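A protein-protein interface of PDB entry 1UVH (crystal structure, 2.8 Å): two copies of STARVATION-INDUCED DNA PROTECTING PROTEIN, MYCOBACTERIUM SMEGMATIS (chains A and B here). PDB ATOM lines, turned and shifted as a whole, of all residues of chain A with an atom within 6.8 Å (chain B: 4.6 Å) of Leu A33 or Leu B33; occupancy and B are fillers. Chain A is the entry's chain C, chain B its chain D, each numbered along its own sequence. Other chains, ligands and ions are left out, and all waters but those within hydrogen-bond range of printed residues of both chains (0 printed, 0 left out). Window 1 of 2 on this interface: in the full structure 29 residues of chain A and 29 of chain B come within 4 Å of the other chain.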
ATOM      1  N   TYR A  28      -0.564  28.885 -19.863  1.00  0.00           N
ATOM      2  CA  TYR A  28      -0.818  28.182 -18.590  1.00  0.00           C
ATOM      3  C   TYR A  28      -2.232  28.462 -18.066  1.00  0.00           C
ATOM      4  O   TYR A  28      -2.987  27.538 -17.809  1.00  0.00           O
ATOM      5  CB  TYR A  28       0.153  28.584 -17.483  1.00  0.00           C
ATOM      6  CG  TYR A  28       1.613  28.296 -17.705  1.00  0.00           C
ATOM      7  CD1 TYR A  28       2.059  27.104 -18.280  1.00  0.00           C
ATOM      8  CD2 TYR A  28       2.564  29.222 -17.292  1.00  0.00           C
ATOM      9  CE1 TYR A  28       3.426  26.856 -18.442  1.00  0.00           C
ATOM     10  CE2 TYR A  28       3.908  29.005 -17.476  1.00  0.00           C
ATOM     11  CZ  TYR A  28       4.341  27.828 -18.034  1.00  0.00           C
ATOM     12  OH  TYR A  28       5.704  27.691 -18.155  1.00  0.00           O
ATOM     13  N   ASN A  29      -2.599  29.723 -17.869  1.00  0.00           N
ATOM     14  CA  ASN A  29      -3.946  29.997 -17.376  1.00  0.00           C
ATOM     15  C   ASN A  29      -5.055  29.255 -18.151  1.00  0.00           C
ATOM     16  O   ASN A  29      -5.967  28.657 -17.580  1.00  0.00           O
ATOM     17  CB  ASN A  29      -4.194  31.465 -17.430  1.00  0.00           C
ATOM     18  CG  ASN A  29      -3.574  32.156 -16.316  1.00  0.00           C
ATOM     19  OD1 ASN A  29      -3.949  31.917 -15.170  1.00  0.00           O
ATOM     20  ND2 ASN A  29      -2.599  33.018 -16.602  1.00  0.00           N
ATOM     21  N   ASP A  30      -4.969  29.295 -19.475  1.00  0.00           N
ATOM     22  CA  ASP A  30      -5.857  28.484 -20.281  1.00  0.00           C
ATOM     23  C   ASP A  30      -5.728  27.036 -19.791  1.00  0.00           C
ATOM     24  O   ASP A  30      -6.701  26.388 -19.502  1.00  0.00           O
ATOM     25  CB  ASP A  30      -5.512  28.595 -21.782  1.00  0.00           C
ATOM     26  CG  ASP A  30      -6.329  27.630 -22.613  1.00  0.00           C
ATOM     27  OD1 ASP A  30      -7.555  27.900 -22.741  1.00  0.00           O
ATOM     28  OD2 ASP A  30      -5.859  26.557 -23.092  1.00  0.00           O
ATOM     29  N   LEU A  31      -4.494  26.572 -19.711  1.00  0.00           N
ATOM     30  CA  LEU A  31      -4.154  25.215 -19.302  1.00  0.00           C
ATOM     31  C   LEU A  31      -4.713  24.794 -17.950  1.00  0.00           C
ATOM     32  O   LEU A  31      -5.199  23.663 -17.775  1.00  0.00           O
ATOM     33  CB  LEU A  31      -2.638  25.079 -19.242  1.00  0.00           C
ATOM     34  CG  LEU A  31      -1.988  23.849 -19.823  1.00  0.00           C
ATOM     35  CD1 LEU A  31      -0.641  23.742 -19.106  1.00  0.00           C
ATOM     36  CD2 LEU A  31      -2.793  22.616 -19.659  1.00  0.00           C
ATOM     37  N   HIS A  32      -4.635  25.672 -16.963  1.00  0.00           N
ATOM     38  CA  HIS A  32      -4.986  25.154 -15.669  1.00  0.00           C
ATOM     39  C   HIS A  32      -6.464  25.008 -15.653  1.00  0.00           C
ATOM     40  O   HIS A  32      -6.967  24.036 -15.134  1.00  0.00           O
ATOM     41  CB  HIS A  32      -4.310  25.790 -14.433  1.00  0.00           C
ATOM     42  CG  HIS A  32      -4.528  27.247 -14.199  1.00  0.00           C
ATOM     43  ND1 HIS A  32      -5.659  27.739 -13.570  1.00  0.00           N
ATOM     44  CD2 HIS A  32      -3.666  28.288 -14.298  1.00  0.00           C
ATOM     45  CE1 HIS A  32      -5.514  29.044 -13.380  1.00  0.00           C
ATOM     46  NE2 HIS A  32      -4.316  29.403 -13.814  1.00  0.00           N
ATOM     47  N   LEU A  33      -7.132  25.890 -16.371  1.00  0.00           N
ATOM     48  CA  LEU A  33      -8.563  25.791 -16.531  1.00  0.00           C
ATOM     49  C   LEU A  33      -8.895  24.562 -17.340  1.00  0.00           C
ATOM     50  O   LEU A  33      -9.631  23.709 -16.872  1.00  0.00           O
ATOM     51  CB  LEU A  33      -9.087  27.035 -17.208  1.00  0.00           C
ATOM     52  CG  LEU A  33      -8.871  28.266 -16.328  1.00  0.00           C
ATOM     53  CD1 LEU A  33      -8.930  29.526 -17.158  1.00  0.00           C
ATOM     54  CD2 LEU A  33      -9.911  28.289 -15.214  1.00  0.00           C
ATOM     55  N   THR A  34      -8.360  24.489 -18.558  1.00  0.00           N
ATOM     56  CA  THR A  34      -8.453  23.304 -19.418  1.00  0.00           C
ATOM     57  C   THR A  34      -8.295  21.988 -18.624  1.00  0.00           C
ATOM     58  O   THR A  34      -9.258  21.227 -18.518  1.00  0.00           O
ATOM     59  CB  THR A  34      -7.412  23.418 -20.500  1.00  0.00           C
ATOM     60  OG1 THR A  34      -7.707  24.549 -21.312  1.00  0.00           O
ATOM     61  CG2 THR A  34      -7.489  22.292 -21.450  1.00  0.00           C
ATOM     62  N   LEU A  35      -7.104  21.734 -18.065  1.00  0.00           N
ATOM     63  CA  LEU A  35      -6.892  20.662 -17.039  1.00  0.00           C
ATOM     64  C   LEU A  35      -8.050  20.514 -16.055  1.00  0.00           C
ATOM     65  O   LEU A  35      -8.659  19.480 -15.912  1.00  0.00           O
ATOM     66  CB  LEU A  35      -5.643  20.957 -16.221  1.00  0.00           C
ATOM     67  CG  LEU A  35      -4.362  20.693 -16.980  1.00  0.00           C
ATOM     68  CD1 LEU A  35      -3.189  21.200 -16.203  1.00  0.00           C
ATOM     69  CD2 LEU A  35      -4.182  19.224 -17.294  1.00  0.00           C
ATOM     70  N   LYS A  36      -8.359  21.576 -15.365  1.00  0.00           N
ATOM     71  CA  LYS A  36      -9.388  21.487 -14.383  1.00  0.00           C
ATOM     72  C   LYS A  36     -10.715  21.055 -15.045  1.00  0.00           C
ATOM     73  O   LYS A  36     -11.445  20.165 -14.527  1.00  0.00           O
ATOM     74  CB  LYS A  36      -9.515  22.818 -13.668  1.00  0.00           C
ATOM     75  CG  LYS A  36     -10.048  22.694 -12.286  1.00  0.00           C
ATOM     76  CD  LYS A  36      -9.132  21.935 -11.275  1.00  0.00           C
ATOM     77  CE  LYS A  36      -9.845  21.800  -9.981  1.00  0.00           C
ATOM     78  NZ  LYS A  36      -9.296  20.723  -9.089  1.00  0.00           N
ATOM     79  N   HIS A  37     -10.998  21.662 -16.215  1.00  0.00           N
ATOM     80  CA  HIS A  37     -12.192  21.363 -17.020  1.00  0.00           C
ATOM     81  C   HIS A  37     -12.230  19.884 -17.383  1.00  0.00           C
ATOM     82  O   HIS A  37     -13.262  19.211 -17.204  1.00  0.00           O
ATOM     83  CB  HIS A  37     -12.224  22.208 -18.305  1.00  0.00           C
ATOM     84  CG  HIS A  37     -13.376  21.865 -19.204  1.00  0.00           C
ATOM     85  ND1 HIS A  37     -13.218  21.183 -20.395  1.00  0.00           N
ATOM     86  CD2 HIS A  37     -14.710  22.030 -19.032  1.00  0.00           C
ATOM     87  CE1 HIS A  37     -14.409  20.969 -20.925  1.00  0.00           C
ATOM     88  NE2 HIS A  37     -15.328  21.465 -20.114  1.00  0.00           N
ATOM     89  N   VAL A  38     -11.090  19.387 -17.864  1.00  0.00           N
ATOM     90  CA  VAL A  38     -10.973  17.990 -18.162  1.00  0.00           C
ATOM     91  C   VAL A  38     -11.267  17.190 -16.928  1.00  0.00           C
ATOM     92  O   VAL A  38     -11.880  16.125 -17.011  1.00  0.00           O
ATOM     93  CB  VAL A  38      -9.581  17.598 -18.618  1.00  0.00           C
ATOM     94  CG1 VAL A  38      -9.455  16.075 -18.715  1.00  0.00           C
ATOM     95  CG2 VAL A  38      -9.224  18.264 -19.937  1.00  0.00           C
ATOM     96  N   HIS A  39     -10.824  17.699 -15.783  1.00  0.00           N
ATOM     97  CA  HIS A  39     -10.700  16.847 -14.601  1.00  0.00           C
ATOM     98  C   HIS A  39     -12.082  16.496 -14.064  1.00  0.00           C
ATOM     99  O   HIS A  39     -12.368  15.349 -13.695  1.00  0.00           O
ATOM    100  CB  HIS A  39      -9.743  17.462 -13.552  1.00  0.00           C
ATOM    101  CG  HIS A  39     -10.218  17.352 -12.140  1.00  0.00           C
ATOM    102  ND1 HIS A  39     -10.317  16.152 -11.477  1.00  0.00           N
ATOM    103  CD2 HIS A  39     -10.609  18.306 -11.258  1.00  0.00           C
ATOM    104  CE1 HIS A  39     -10.753  16.379 -10.252  1.00  0.00           C
ATOM    105  NE2 HIS A  39     -10.951  17.669 -10.092  1.00  0.00           N
ATOM    106  N   TRP A  40     -12.962  17.470 -14.095  1.00  0.00           N
ATOM    107  CA  TRP A  40     -14.268  17.222 -13.562  1.00  0.00           C
ATOM    108  C   TRP A  40     -15.251  16.796 -14.670  1.00  0.00           C
ATOM    109  O   TRP A  40     -16.419  16.542 -14.392  1.00  0.00           O
ATOM    110  CB  TRP A  40     -14.724  18.388 -12.671  1.00  0.00           C
ATOM    111  CG  TRP A  40     -14.682  19.719 -13.276  1.00  0.00           C
ATOM    112  CD1 TRP A  40     -15.202  20.077 -14.479  1.00  0.00           C
ATOM    113  CD2 TRP A  40     -14.123  20.918 -12.713  1.00  0.00           C
ATOM    114  NE1 TRP A  40     -15.017  21.424 -14.698  1.00  0.00           N
ATOM    115  CE2 TRP A  40     -14.357  21.968 -13.634  1.00  0.00           C
ATOM    116  CE3 TRP A  40     -13.473  21.219 -11.527  1.00  0.00           C
ATOM    117  CZ2 TRP A  40     -13.949  23.278 -13.417  1.00  0.00           C
ATOM    118  CZ3 TRP A  40     -13.086  22.546 -11.310  1.00  0.00           C
ATOM    119  CH2 TRP A  40     -13.317  23.549 -12.259  1.00  0.00           C
ATOM    120  N   VAL A  58      -2.651  20.539 -12.189  1.00  0.00           N
ATOM    121  CA  VAL A  58      -3.330  21.803 -12.126  1.00  0.00           C
ATOM    122  C   VAL A  58      -2.525  22.679 -11.251  1.00  0.00           C
ATOM    123  O   VAL A  58      -2.157  23.767 -11.607  1.00  0.00           O
ATOM    124  CB  VAL A  58      -4.674  21.709 -11.521  1.00  0.00           C
ATOM    125  CG1 VAL A  58      -5.190  23.097 -11.261  1.00  0.00           C
ATOM    126  CG2 VAL A  58      -5.596  21.009 -12.428  1.00  0.00           C
ATOM    127  N   ARG A  62      -0.730  26.218 -12.165  1.00  0.00           N
ATOM    128  CA  ARG A  62      -1.256  27.420 -11.510  1.00  0.00           C
ATOM    129  C   ARG A  62      -0.110  28.212 -10.888  1.00  0.00           C
ATOM    130  O   ARG A  62      -0.117  29.441 -10.931  1.00  0.00           O
ATOM    131  CB  ARG A  62      -2.268  27.131 -10.403  1.00  0.00           C
ATOM    132  CG  ARG A  62      -3.510  26.314 -10.743  1.00  0.00           C
ATOM    133  CD  ARG A  62      -4.779  26.768  -9.948  1.00  0.00           C
ATOM    134  NE  ARG A  62      -5.988  26.029 -10.325  1.00  0.00           N
ATOM    135  CZ  ARG A  62      -6.866  25.493  -9.497  1.00  0.00           C
ATOM    136  NH1 ARG A  62      -6.735  25.566  -8.203  1.00  0.00           N
ATOM    137  NH2 ARG A  62      -7.882  24.821  -9.955  1.00  0.00           N
ATOM    138  N   GLY A  81      -3.726  38.612 -16.507  1.00  0.00           N
ATOM    139  CA  GLY A  81      -4.286  37.322 -16.092  1.00  0.00           C
ATOM    140  C   GLY A  81      -5.819  37.219 -15.961  1.00  0.00           C
ATOM    141  O   GLY A  81      -6.352  36.421 -15.183  1.00  0.00           O
ATOM    142  N   THR A  82      -6.525  38.043 -16.731  1.00  0.00           N
ATOM    143  CA  THR A  82      -7.984  38.048 -16.762  1.00  0.00           C
ATOM    144  C   THR A  82      -8.366  37.274 -17.991  1.00  0.00           C
ATOM    145  O   THR A  82      -7.636  37.258 -18.980  1.00  0.00           O
ATOM    146  CB  THR A  82      -8.504  39.455 -16.896  1.00  0.00           C
ATOM    147  OG1 THR A  82      -7.802  40.100 -17.966  1.00  0.00           O
ATOM    148  CG2 THR A  82      -8.144  40.286 -15.673  1.00  0.00           C
ATOM    149  N   PRO A  83      -9.513  36.631 -17.954  1.00  0.00           N
ATOM    150  CA  PRO A  83      -9.858  35.694 -19.010  1.00  0.00           C
ATOM    151  C   PRO A  83      -9.870  36.386 -20.373  1.00  0.00           C
ATOM    152  O   PRO A  83      -9.627  35.746 -21.409  1.00  0.00           O
ATOM    153  CB  PRO A  83     -11.237  35.191 -18.603  1.00  0.00           C
ATOM    154  CG  PRO A  83     -11.679  35.989 -17.488  1.00  0.00           C
ATOM    155  CD  PRO A  83     -10.560  36.756 -16.939  1.00  0.00           C
ATOM    156  N   ILE A  86      -6.427  36.368 -21.800  1.00  0.00           N
ATOM    157  CA  ILE A  86      -5.878  35.085 -22.223  1.00  0.00           C
ATOM    158  C   ILE A  86      -6.401  34.743 -23.605  1.00  0.00           C
ATOM    159  O   ILE A  86      -5.645  34.345 -24.460  1.00  0.00           O
ATOM    160  CB  ILE A  86      -6.060  33.958 -21.119  1.00  0.00           C
ATOM    161  CG1 ILE A  86      -7.198  32.986 -21.400  1.00  0.00           C
ATOM    162  CG2 ILE A  86      -6.263  34.582 -19.700  1.00  0.00           C
ATOM    163  CD1 ILE A  86      -7.524  32.149 -20.170  1.00  0.00           C
ATOM    164  N   ASN B  29     -14.355  31.094 -11.685  1.00  0.00           N
ATOM    165  CA  ASN B  29     -13.152  31.047 -12.509  1.00  0.00           C
ATOM    166  C   ASN B  29     -12.661  32.436 -13.014  1.00  0.00           C
ATOM    167  O   ASN B  29     -11.467  32.690 -13.150  1.00  0.00           O
ATOM    168  CB  ASN B  29     -13.354  30.119 -13.659  1.00  0.00           C
ATOM    169  CG  ASN B  29     -13.494  28.713 -13.232  1.00  0.00           C
ATOM    170  OD1 ASN B  29     -12.670  28.207 -12.448  1.00  0.00           O
ATOM    171  ND2 ASN B  29     -14.526  28.033 -13.743  1.00  0.00           N
ATOM    172  N   ASP B  30     -13.605  33.339 -13.296  1.00  0.00           N
ATOM    173  CA  ASP B  30     -13.256  34.719 -13.618  1.00  0.00           C
ATOM    174  C   ASP B  30     -12.609  35.247 -12.359  1.00  0.00           C
ATOM    175  O   ASP B  30     -11.458  35.606 -12.365  1.00  0.00           O
ATOM    176  CB  ASP B  30     -14.477  35.576 -14.041  1.00  0.00           C
ATOM    177  CG  ASP B  30     -14.104  37.057 -14.253  1.00  0.00           C
ATOM    178  OD1 ASP B  30     -13.372  37.348 -15.243  1.00  0.00           O
ATOM    179  OD2 ASP B  30     -14.468  37.983 -13.464  1.00  0.00           O
ATOM    180  N   LEU B  31     -13.364  35.232 -11.278  1.00  0.00           N
ATOM    181  CA  LEU B  31     -12.844  35.598  -9.986  1.00  0.00           C
ATOM    182  C   LEU B  31     -11.434  35.111  -9.701  1.00  0.00           C
ATOM    183  O   LEU B  31     -10.602  35.870  -9.213  1.00  0.00           O
ATOM    184  CB  LEU B  31     -13.749  35.080  -8.897  1.00  0.00           C
ATOM    185  CG  LEU B  31     -14.149  36.110  -7.869  1.00  0.00           C
ATOM    186  CD1 LEU B  31     -14.576  35.350  -6.614  1.00  0.00           C
ATOM    187  CD2 LEU B  31     -13.078  37.086  -7.551  1.00  0.00           C
ATOM    188  N   HIS B  32     -11.123  33.852  -9.960  1.00  0.00           N
ATOM    189  CA  HIS B  32      -9.904  33.408  -9.338  1.00  0.00           C
ATOM    190  C   HIS B  32      -8.775  33.960 -10.167  1.00  0.00           C
ATOM    191  O   HIS B  32      -7.791  34.456  -9.634  1.00  0.00           O
ATOM    192  CB  HIS B  32      -9.869  31.947  -8.862  1.00  0.00           C
ATOM    193  CG  HIS B  32      -9.881  30.898  -9.914  1.00  0.00           C
ATOM    194  ND1 HIS B  32      -8.781  30.620 -10.712  1.00  0.00           N
ATOM    195  CD2 HIS B  32     -10.791  29.921 -10.163  1.00  0.00           C
ATOM    196  CE1 HIS B  32      -9.059  29.568 -11.476  1.00  0.00           C
ATOM    197  NE2 HIS B  32     -10.271  29.124 -11.159  1.00  0.00           N
ATOM    198  N   LEU B  33      -9.004  34.024 -11.463  1.00  0.00           N
ATOM    199  CA  LEU B  33      -8.033  34.612 -12.357  1.00  0.00           C
ATOM    200  C   LEU B  33      -7.886  36.084 -12.034  1.00  0.00           C
ATOM    201  O   LEU B  33      -6.801  36.565 -11.797  1.00  0.00           O
ATOM    202  CB  LEU B  33      -8.504  34.408 -13.779  1.00  0.00           C
ATOM    203  CG  LEU B  33      -8.461  32.948 -14.241  1.00  0.00           C
ATOM    204  CD1 LEU B  33      -9.284  32.772 -15.502  1.00  0.00           C
ATOM    205  CD2 LEU B  33      -7.024  32.536 -14.484  1.00  0.00           C
ATOM    206  N   THR B  34      -9.011  36.782 -12.026  1.00  0.00           N
ATOM    207  CA  THR B  34      -9.098  38.164 -11.586  1.00  0.00           C
ATOM    208  C   THR B  34      -8.314  38.458 -10.306  1.00  0.00           C
ATOM    209  O   THR B  34      -7.429  39.345 -10.318  1.00  0.00           O
ATOM    210  CB  THR B  34     -10.538  38.521 -11.422  1.00  0.00           C
ATOM    211  OG1 THR B  34     -11.117  38.603 -12.718  1.00  0.00           O
ATOM    212  CG2 THR B  34     -10.703  39.876 -10.836  1.00  0.00           C
ATOM    213  N   LEU B  35      -8.613  37.730  -9.223  1.00  0.00           N
ATOM    214  CA  LEU B  35      -7.823  37.837  -7.960  1.00  0.00           C
ATOM    215  C   LEU B  35      -6.324  37.689  -8.240  1.00  0.00           C
ATOM    216  O   LEU B  35      -5.515  38.557  -7.970  1.00  0.00           O
ATOM    217  CB  LEU B  35      -8.250  36.772  -6.973  1.00  0.00           C
ATOM    218  CG  LEU B  35      -9.560  37.092  -6.278  1.00  0.00           C
ATOM    219  CD1 LEU B  35     -10.205  35.853  -5.704  1.00  0.00           C
ATOM    220  CD2 LEU B  35      -9.342  38.071  -5.191  1.00  0.00           C
ATOM    221  N   LYS B  36      -5.965  36.600  -8.863  1.00  0.00           N
ATOM    222  CA  LYS B  36      -4.582  36.385  -9.130  1.00  0.00           C
ATOM    223  C   LYS B  36      -3.984  37.562  -9.908  1.00  0.00           C
ATOM    224  O   LYS B  36      -2.884  38.055  -9.540  1.00  0.00           O
ATOM    225  CB  LYS B  36      -4.389  35.053  -9.839  1.00  0.00           C
ATOM    226  CG  LYS B  36      -3.205  34.265  -9.304  1.00  0.00           C
ATOM    227  CD  LYS B  36      -3.226  33.952  -7.791  1.00  0.00           C
ATOM    228  CE  LYS B  36      -1.894  33.426  -7.338  1.00  0.00           C
ATOM    229  NZ  LYS B  36      -1.448  32.410  -8.324  1.00  0.00           N
ATOM    230  N   HIS B  37      -4.748  38.051 -10.915  1.00  0.00           N
ATOM    231  CA  HIS B  37      -4.356  39.193 -11.780  1.00  0.00           C
ATOM    232  C   HIS B  37      -4.042  40.422 -10.961  1.00  0.00           C
ATOM    233  O   HIS B  37      -3.004  41.085 -11.174  1.00  0.00           O
ATOM    234  CB  HIS B  37      -5.438  39.588 -12.804  1.00  0.00           C
ATOM    235  CG  HIS B  37      -5.024  40.758 -13.660  1.00  0.00           C
ATOM    236  ND1 HIS B  37      -5.647  41.986 -13.612  1.00  0.00           N
ATOM    237  CD2 HIS B  37      -3.974  40.907 -14.503  1.00  0.00           C
ATOM    238  CE1 HIS B  37      -5.012  42.830 -14.406  1.00  0.00           C
ATOM    239  NE2 HIS B  37      -3.993  42.199 -14.955  1.00  0.00           N
ATOM    240  N   GLY B  81     -15.459  24.713 -18.022  1.00  0.00           N
ATOM    241  CA  GLY B  81     -14.377  25.308 -17.268  1.00  0.00           C
ATOM    242  C   GLY B  81     -13.394  26.138 -18.074  1.00  0.00           C
ATOM    243  O   GLY B  81     -12.582  26.849 -17.501  1.00  0.00           O
ATOM    244  N   PRO B  83     -11.831  29.048 -20.650  1.00  0.00           N
ATOM    245  CA  PRO B  83     -12.025  30.480 -20.793  1.00  0.00           C
ATOM    246  C   PRO B  83     -13.155  30.820 -21.779  1.00  0.00           C
ATOM    247  O   PRO B  83     -13.873  31.829 -21.602  1.00  0.00           O
ATOM    248  CB  PRO B  83     -10.680  30.954 -21.333  1.00  0.00           C
ATOM    249  CG  PRO B  83      -9.949  29.744 -21.716  1.00  0.00           C
ATOM    250  CD  PRO B  83     -10.434  28.664 -20.866  1.00  0.00           C
ATOM    251  N   ILE B  86     -16.359  30.746 -19.935  1.00  0.00           N
ATOM    252  CA  ILE B  86     -16.617  31.737 -18.898  1.00  0.00           C
ATOM    253  C   ILE B  86     -16.979  33.043 -19.538  1.00  0.00           C
ATOM    254  O   ILE B  86     -17.983  33.606 -19.199  1.00  0.00           O
ATOM    255  CB  ILE B  86     -15.482  31.828 -17.808  1.00  0.00           C
ATOM    256  CG1 ILE B  86     -14.198  32.457 -18.330  1.00  0.00           C
ATOM    257  CG2 ILE B  86     -15.136  30.408 -17.259  1.00  0.00           C
ATOM    258  CD1 ILE B  86     -13.069  32.392 -17.308  1.00  0.00           C
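The backbone carbonyl oxygen (O) of Leu B33 lies close to the backbone carbonyl oxygen (O) of Gly A81, 3.4 Å away.
The side-chain amide oxygen (OD1) of Asn A29 sits at hydrogen-bond distance from a ring nitrogen (NE2) of His A32 (2.9 Å). The backbone carbonyl oxygen (O) of Asp A30 lies within hydrogen-bond range of the side-chain hydroxyl (OG1) of Thr A34, 2.8 Å away. OD1 of Asn B29 lies within hydrogen-bond range of NE2 of His B32 (2.9 Å). The backbone carbonyl oxygen (O) of Asp B30 is in hydrogen-bond range of the side-chain hydroxyl (OG1) of Thr B34, at 3.0 Å.
Among the printed residues, merely in contact across the chains: Asn A29 with Leu B33 (3.2 Å), Asp A30 with Pro B83 (3.2 Å), His A32 with Leu B33 (3.96 Å), Leu A33 with Asn B29 (3.9 Å), Leu A33 with Leu B33 (3.7 Å), Leu A33 with Gly B81 (3.5 Å), His A37 with Gly B81 (3.0 Å), Gly A81 with His B37 (3.1 Å), Thr A82 with His B37 (3.7 Å), Pro A83 with Asp B30 (3.1 Å), Pro A83 with Ile B86 (3.6 Å) and Ile A86 with Pro B83 (3.6 Å).
Printed residues of chain B within 4 Å of Asp A30: Pro B83 (3.2 Å). Of the printed residues of chain B, His A32 touches Leu B33. Thr A34 touches none of the printed residues of chain B. His A39 touches none of the printed residues of chain B. Of the printed residues of chain B, Pro A83 touches Asp B30 (3.1 Å) and Ile B86 (3.6 Å). Printed residues of chain A within 4 Å of Asn B29: Leu A33. Leu B33 touches just these residues of chain A: Asn A29 (3.2 Å), His A32 (3.96 Å), Leu A33 (3.7 Å) and Gly A81 (3.3 Å). Of the printed residues of chain A, His B37 touches Gly A81 (3.1 Å) and Thr A82 (3.7 Å).
Of the 19 printed residues of chain A, 9 touch a printed residue of chain B. Printed residues of chain A that touch a printed residue of chain B: Asn A29, Asp A30, His A32, Leu A33, His A37, Gly A81, Thr A82, Pro A83 and Ile A86. Hydrophobic or aromatic side chains of chain A that line the printed part of chain B: His A32, Leu A33, His A37, Pro A83 and Ile A86. Printed residues of chain B that touch a printed residue of chain A: Asn B29, Asp B30, Leu B33, His B37, Gly B81, Pro B83 and Ile B86.
His A32 touches Leu B33, but with the chains exchanged Leu A33 does not touch His B32 (4.04 Å). Leu A33 touches Gly B81, and with the chains exchanged Gly A81 touches Leu B33. His A37 touches Gly B81, and with the chains exchanged Gly A81 touches His B37. Pro A83 touches Ile B86, and with the chains exchanged Ile A86 touches Pro B83. Positions printed for both chains: 29, 30, 31, 32, 33, 34, 35, 36, 37, 81, 83 and 86. Of the 13 pairs that touch across the chains among the printed residues, 11 have their exchanged pair printed and touching as well.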
